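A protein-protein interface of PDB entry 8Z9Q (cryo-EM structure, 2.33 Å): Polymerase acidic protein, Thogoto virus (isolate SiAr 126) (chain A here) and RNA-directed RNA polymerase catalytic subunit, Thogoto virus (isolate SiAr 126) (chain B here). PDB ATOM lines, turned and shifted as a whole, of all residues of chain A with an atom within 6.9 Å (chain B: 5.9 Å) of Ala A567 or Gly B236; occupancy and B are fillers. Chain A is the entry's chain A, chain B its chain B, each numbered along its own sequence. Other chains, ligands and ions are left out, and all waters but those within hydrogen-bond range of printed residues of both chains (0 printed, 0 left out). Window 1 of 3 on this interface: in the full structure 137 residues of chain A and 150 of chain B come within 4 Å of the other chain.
OE1 of Glu A563 sits at hydrogen-bond distance from N of Gly B236 (3.3 Å).
NE of Arg B235 is in salt-bridge range of OE2 of Glu A563.
O of Leu B19 is in hydrogen-bond range of NE of Arg A570 (3.1 Å).
Among the printed residues, pairs that only touch across the chains: Pro A560 with Arg B237 (3.8 Å), Pro A560 with Leu B238 (3.4 Å), Gln A561 with Leu B238 (3.8 Å), Glu A563 with Glu B234 (3.9 Å), Leu A566 with Leu B19 (3.5 Å), Ala A567 with Gly B236 (3.3 Å) and Met A569 with Leu B19 (3.99 Å).
Ala A567 touches one residue of chain B.
Gly B236 touches just these residues of chain A: Glu A563 (3.3 Å) and Ala A567 (3.3 Å).
Printed residues of chain B within 4 Å of Leu A566: Leu B19 (3.5 Å).
Printed residues of chain A within 4 Å of Arg B235: Glu A563 (3.3 Å).
Of the printed residues of chain A, Arg B237 touches Pro A560.
Val A597 touches none of the printed residues of chain B.
Asn A568 touches none of the printed residues of chain B.
The nearest residue of chain A that does not touch Gly B236 is Gly A564 (4.2 Å).
The nearest printed residue of chain A that does not touch Glu B234 is Pro A560 (7.4 Å).
Of the 14 printed residues of chain A, 7 touch a printed residue of chain B.
Printed residues of chain A that touch a printed residue of chain B: Pro A560, Gln A561, Glu A563, Leu A566, Ala A567, Met A569 and Arg A570.
Hydrophobic or aromatic side chains of chain A within 4 Å of the printed part of chain B: Pro A560, Leu A566 and Ala A567.
Among the printed residues, 10 pairs touch across the chains.
Among the printed residues, Asp or Glu carboxylates within 4 Å of a Lys or Arg side-chain nitrogen of the other chain: Glu A563 with Arg B235 (3.3 Å).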
ATOM      1  N   PRO A 560     -22.262  29.920   0.909  1.00  0.00           N
ATOM      2  CA  PRO A 560     -23.228  28.808   0.923  1.00  0.00           C
ATOM      3  C   PRO A 560     -23.192  27.946  -0.327  1.00  0.00           C
ATOM      4  O   PRO A 560     -23.387  26.727  -0.226  1.00  0.00           O
ATOM      5  CB  PRO A 560     -24.575  29.527   1.080  1.00  0.00           C
ATOM      6  CG  PRO A 560     -24.232  30.761   1.815  1.00  0.00           C
ATOM      7  CD  PRO A 560     -22.918  31.195   1.254  1.00  0.00           C
ATOM      8  N   GLN A 561     -22.939  28.534  -1.499  1.00  0.00           N
ATOM      9  CA  GLN A 561     -22.847  27.734  -2.715  1.00  0.00           C
ATOM     10  C   GLN A 561     -21.701  26.735  -2.633  1.00  0.00           C
ATOM     11  O   GLN A 561     -21.868  25.566  -2.992  1.00  0.00           O
ATOM     12  CB  GLN A 561     -22.679  28.634  -3.938  1.00  0.00           C
ATOM     13  CG  GLN A 561     -23.585  29.848  -3.958  1.00  0.00           C
ATOM     14  CD  GLN A 561     -23.427  30.661  -5.222  1.00  0.00           C
ATOM     15  OE1 GLN A 561     -22.981  30.151  -6.248  1.00  0.00           O
ATOM     16  NE2 GLN A 561     -23.788  31.935  -5.156  1.00  0.00           N
ATOM     17  N   MET A 562     -20.536  27.171  -2.150  1.00  0.00           N
ATOM     18  CA  MET A 562     -19.388  26.273  -2.051  1.00  0.00           C
ATOM     19  C   MET A 562     -19.674  25.103  -1.118  1.00  0.00           C
ATOM     20  O   MET A 562     -19.395  23.945  -1.451  1.00  0.00           O
ATOM     21  CB  MET A 562     -18.157  27.047  -1.578  1.00  0.00           C
ATOM     22  CG  MET A 562     -16.895  26.202  -1.464  1.00  0.00           C
ATOM     23  SD  MET A 562     -16.303  25.539  -3.029  1.00  0.00           S
ATOM     24  CE  MET A 562     -15.617  27.011  -3.780  1.00  0.00           C
ATOM     25  N   GLU A 563     -20.237  25.383   0.059  1.00  0.00           N
ATOM     26  CA  GLU A 563     -20.462  24.313   1.025  1.00  0.00           C
ATOM     27  C   GLU A 563     -21.563  23.366   0.568  1.00  0.00           C
ATOM     28  O   GLU A 563     -21.439  22.147   0.731  1.00  0.00           O
ATOM     29  CB  GLU A 563     -20.791  24.889   2.397  1.00  0.00           C
ATOM     30  CG  GLU A 563     -19.639  25.623   3.039  1.00  0.00           C
ATOM     31  CD  GLU A 563     -20.015  26.181   4.383  1.00  0.00           C
ATOM     32  OE1 GLU A 563     -21.208  26.088   4.733  1.00  0.00           O
ATOM     33  OE2 GLU A 563     -19.127  26.704   5.087  1.00  0.00           O
ATOM     34  N   GLY A 564     -22.647  23.902   0.003  1.00  0.00           N
ATOM     35  CA  GLY A 564     -23.667  23.031  -0.557  1.00  0.00           C
ATOM     36  C   GLY A 564     -23.127  22.166  -1.678  1.00  0.00           C
ATOM     37  O   GLY A 564     -23.401  20.962  -1.737  1.00  0.00           O
ATOM     38  N   PHE A 565     -22.322  22.761  -2.563  1.00  0.00           N
ATOM     39  CA  PHE A 565     -21.731  22.012  -3.663  1.00  0.00           C
ATOM     40  C   PHE A 565     -20.843  20.893  -3.145  1.00  0.00           C
ATOM     41  O   PHE A 565     -20.910  19.767  -3.638  1.00  0.00           O
ATOM     42  CB  PHE A 565     -20.944  22.965  -4.570  1.00  0.00           C
ATOM     43  CG  PHE A 565     -20.113  22.277  -5.622  1.00  0.00           C
ATOM     44  CD1 PHE A 565     -18.812  21.881  -5.357  1.00  0.00           C
ATOM     45  CD2 PHE A 565     -20.632  22.041  -6.881  1.00  0.00           C
ATOM     46  CE1 PHE A 565     -18.054  21.252  -6.323  1.00  0.00           C
ATOM     47  CE2 PHE A 565     -19.876  21.415  -7.851  1.00  0.00           C
ATOM     48  CZ  PHE A 565     -18.586  21.022  -7.572  1.00  0.00           C
ATOM     49  N   LEU A 566     -20.011  21.176  -2.142  1.00  0.00           N
ATOM     50  CA  LEU A 566     -19.118  20.142  -1.628  1.00  0.00           C
ATOM     51  C   LEU A 566     -19.894  19.040  -0.914  1.00  0.00           C
ATOM     52  O   LEU A 566     -19.621  17.847  -1.113  1.00  0.00           O
ATOM     53  CB  LEU A 566     -18.083  20.769  -0.698  1.00  0.00           C
ATOM     54  CG  LEU A 566     -17.037  21.634  -1.404  1.00  0.00           C
ATOM     55  CD1 LEU A 566     -16.229  22.433  -0.397  1.00  0.00           C
ATOM     56  CD2 LEU A 566     -16.133  20.780  -2.274  1.00  0.00           C
ATOM     57  N   ALA A 567     -20.876  19.421  -0.093  1.00  0.00           N
ATOM     58  CA  ALA A 567     -21.666  18.436   0.633  1.00  0.00           C
ATOM     59  C   ALA A 567     -22.455  17.541  -0.310  1.00  0.00           C
ATOM     60  O   ALA A 567     -22.694  16.370   0.005  1.00  0.00           O
ATOM     61  CB  ALA A 567     -22.607  19.138   1.611  1.00  0.00           C
ATOM     62  N   ASN A 568     -22.865  18.064  -1.465  1.00  0.00           N
ATOM     63  CA  ASN A 568     -23.610  17.247  -2.412  1.00  0.00           C
ATOM     64  C   ASN A 568     -22.722  16.541  -3.431  1.00  0.00           C
ATOM     65  O   ASN A 568     -23.171  15.572  -4.050  1.00  0.00           O
ATOM     66  CB  ASN A 568     -24.656  18.106  -3.121  1.00  0.00           C
ATOM     67  CG  ASN A 568     -25.672  18.685  -2.157  1.00  0.00           C
ATOM     68  OD1 ASN A 568     -26.390  17.949  -1.483  1.00  0.00           O
ATOM     69  ND2 ASN A 568     -25.724  20.007  -2.076  1.00  0.00           N
ATOM     70  N   MET A 569     -21.481  16.996  -3.621  1.00  0.00           N
ATOM     71  CA  MET A 569     -20.512  16.257  -4.420  1.00  0.00           C
ATOM     72  C   MET A 569     -19.826  15.147  -3.652  1.00  0.00           C
ATOM     73  O   MET A 569     -19.181  14.303  -4.276  1.00  0.00           O
ATOM     74  CB  MET A 569     -19.435  17.183  -4.994  1.00  0.00           C
ATOM     75  CG  MET A 569     -19.916  18.183  -6.017  1.00  0.00           C
ATOM     76  SD  MET A 569     -20.601  17.318  -7.436  1.00  0.00           S
ATOM     77  CE  MET A 569     -19.115  16.602  -8.126  1.00  0.00           C
ATOM     78  N   ARG A 570     -19.919  15.132  -2.322  1.00  0.00           N
ATOM     79  CA  ARG A 570     -19.367  13.994  -1.592  1.00  0.00           C
ATOM     80  C   ARG A 570     -20.047  12.691  -2.007  1.00  0.00           C
ATOM     81  O   ARG A 570     -19.380  11.665  -2.196  1.00  0.00           O
ATOM     82  CB  ARG A 570     -19.482  14.225  -0.087  1.00  0.00           C
ATOM     83  CG  ARG A 570     -18.572  15.331   0.419  1.00  0.00           C
ATOM     84  CD  ARG A 570     -18.806  15.651   1.883  1.00  0.00           C
ATOM     85  NE  ARG A 570     -18.510  17.047   2.176  1.00  0.00           N
ATOM     86  CZ  ARG A 570     -19.184  17.790   3.042  1.00  0.00           C
ATOM     87  NH1 ARG A 570     -20.197  17.296   3.735  1.00  0.00           N
ATOM     88  NH2 ARG A 570     -18.834  19.061   3.217  1.00  0.00           N
ATOM     89  N   ARG A 571     -21.370  12.722  -2.187  1.00  0.00           N
ATOM     90  CA  ARG A 571     -22.101  11.534  -2.625  1.00  0.00           C
ATOM     91  C   ARG A 571     -21.678  11.100  -4.025  1.00  0.00           C
ATOM     92  O   ARG A 571     -21.496   9.907  -4.288  1.00  0.00           O
ATOM     93  CB  ARG A 571     -23.604  11.803  -2.578  1.00  0.00           C
ATOM     94  CG  ARG A 571     -24.158  11.959  -1.175  1.00  0.00           C
ATOM     95  CD  ARG A 571     -25.671  12.025  -1.190  1.00  0.00           C
ATOM     96  NE  ARG A 571     -26.138  13.206  -1.903  1.00  0.00           N
ATOM     97  CZ  ARG A 571     -26.326  14.391  -1.339  1.00  0.00           C
ATOM     98  NH1 ARG A 571     -26.115  14.583  -0.048  1.00  0.00           N
ATOM     99  NH2 ARG A 571     -26.735  15.409  -2.089  1.00  0.00           N
ATOM    100  N   LEU A 572     -21.522  12.056  -4.942  1.00  0.00           N
ATOM    101  CA  LEU A 572     -21.130  11.703  -6.303  1.00  0.00           C
ATOM    102  C   LEU A 572     -19.685  11.224  -6.366  1.00  0.00           C
ATOM    103  O   LEU A 572     -19.358  10.353  -7.176  1.00  0.00           O
ATOM    104  CB  LEU A 572     -21.342  12.891  -7.237  1.00  0.00           C
ATOM    105  CG  LEU A 572     -22.796  13.329  -7.419  1.00  0.00           C
ATOM    106  CD1 LEU A 572     -22.878  14.568  -8.289  1.00  0.00           C
ATOM    107  CD2 LEU A 572     -23.625  12.199  -8.004  1.00  0.00           C
ATOM    108  N   VAL A 597     -26.552  19.147  -6.537  1.00  0.00           N
ATOM    109  CA  VAL A 597     -25.346  19.902  -6.857  1.00  0.00           C
ATOM    110  C   VAL A 597     -25.674  21.100  -7.739  1.00  0.00           C
ATOM    111  O   VAL A 597     -25.213  22.219  -7.486  1.00  0.00           O
ATOM    112  CB  VAL A 597     -24.307  18.983  -7.524  1.00  0.00           C
ATOM    113  CG1 VAL A 597     -23.084  19.780  -7.920  1.00  0.00           C
ATOM    114  CG2 VAL A 597     -23.942  17.839  -6.599  1.00  0.00           C
ATOM    115  N   LEU B  19     -12.984  17.577   0.126  1.00  0.00           N
ATOM    116  CA  LEU B  19     -14.211  18.247  -0.282  1.00  0.00           C
ATOM    117  C   LEU B  19     -14.860  18.931   0.913  1.00  0.00           C
ATOM    118  O   LEU B  19     -16.039  18.705   1.202  1.00  0.00           O
ATOM    119  CB  LEU B  19     -15.188  17.256  -0.920  1.00  0.00           C
ATOM    120  CG  LEU B  19     -14.632  16.241  -1.920  1.00  0.00           C
ATOM    121  CD1 LEU B  19     -15.764  15.471  -2.574  1.00  0.00           C
ATOM    122  CD2 LEU B  19     -13.780  16.928  -2.970  1.00  0.00           C
ATOM    123  N   GLU B 234     -23.626  26.772  10.649  1.00  0.00           N
ATOM    124  CA  GLU B 234     -23.984  25.494  10.053  1.00  0.00           C
ATOM    125  C   GLU B 234     -23.349  25.389   8.674  1.00  0.00           C
ATOM    126  O   GLU B 234     -23.457  26.314   7.863  1.00  0.00           O
ATOM    127  CB  GLU B 234     -25.502  25.343   9.959  1.00  0.00           C
ATOM    128  CG  GLU B 234     -25.965  23.912   9.753  1.00  0.00           C
ATOM    129  CD  GLU B 234     -27.437  23.821   9.413  1.00  0.00           C
ATOM    130  OE1 GLU B 234     -28.049  24.870   9.122  1.00  0.00           O
ATOM    131  OE2 GLU B 234     -27.984  22.699   9.440  1.00  0.00           O
ATOM    132  N   ARG B 235     -22.687  24.266   8.416  1.00  0.00           N
ATOM    133  CA  ARG B 235     -21.933  24.061   7.191  1.00  0.00           C
ATOM    134  C   ARG B 235     -22.552  22.947   6.359  1.00  0.00           C
ATOM    135  O   ARG B 235     -23.211  22.046   6.886  1.00  0.00           O
ATOM    136  CB  ARG B 235     -20.471  23.722   7.498  1.00  0.00           C
ATOM    137  CG  ARG B 235     -19.738  24.791   8.284  1.00  0.00           C
ATOM    138  CD  ARG B 235     -18.269  24.448   8.443  1.00  0.00           C
ATOM    139  NE  ARG B 235     -17.433  25.191   7.509  1.00  0.00           N
ATOM    140  CZ  ARG B 235     -16.734  26.272   7.826  1.00  0.00           C
ATOM    141  NH1 ARG B 235     -16.743  26.766   9.053  1.00  0.00           N
ATOM    142  NH2 ARG B 235     -16.008  26.873   6.889  1.00  0.00           N
ATOM    143  N   GLY B 236     -22.334  23.021   5.050  1.00  0.00           N
ATOM    144  CA  GLY B 236     -22.794  21.989   4.146  1.00  0.00           C
ATOM    145  C   GLY B 236     -24.177  22.188   3.577  1.00  0.00           C
ATOM    146  O   GLY B 236     -24.747  21.235   3.034  1.00  0.00           O
ATOM    147  N   ARG B 237     -24.741  23.387   3.682  1.00  0.00           N
ATOM    148  CA  ARG B 237     -26.077  23.660   3.176  1.00  0.00           C
ATOM    149  C   ARG B 237     -26.090  24.971   2.407  1.00  0.00           C
ATOM    150  O   ARG B 237     -25.451  25.947   2.811  1.00  0.00           O
ATOM    151  CB  ARG B 237     -27.105  23.721   4.310  1.00  0.00           C
ATOM    152  CG  ARG B 237     -27.336  22.398   5.010  1.00  0.00           C
ATOM    153  CD  ARG B 237     -28.375  22.542   6.101  1.00  0.00           C
ATOM    154  NE  ARG B 237     -29.670  22.917   5.547  1.00  0.00           N
ATOM    155  CZ  ARG B 237     -30.564  22.055   5.084  1.00  0.00           C
ATOM    156  NH1 ARG B 237     -30.339  20.751   5.096  1.00  0.00           N
ATOM    157  NH2 ARG B 237     -31.716  22.513   4.601  1.00  0.00           N
ATOM    158  N   LEU B 238     -26.826  24.984   1.296  1.00  0.00           N
ATOM    159  CA  LEU B 238     -27.010  26.211   0.535  1.00  0.00           C
ATOM    160  C   LEU B 238     -27.998  27.154   1.209  1.00  0.00           C
ATOM    161  O   LEU B 238     -27.826  28.377   1.142  1.00  0.00           O
ATOM    162  CB  LEU B 238     -27.479  25.879  -0.883  1.00  0.00           C
ATOM    163  CG  LEU B 238     -27.848  27.050  -1.795  1.00  0.00           C
ATOM    164  CD1 LEU B 238     -26.608  27.838  -2.182  1.00  0.00           C
ATOM    165  CD2 LEU B 238     -28.583  26.559  -3.030  1.00  0.00           C
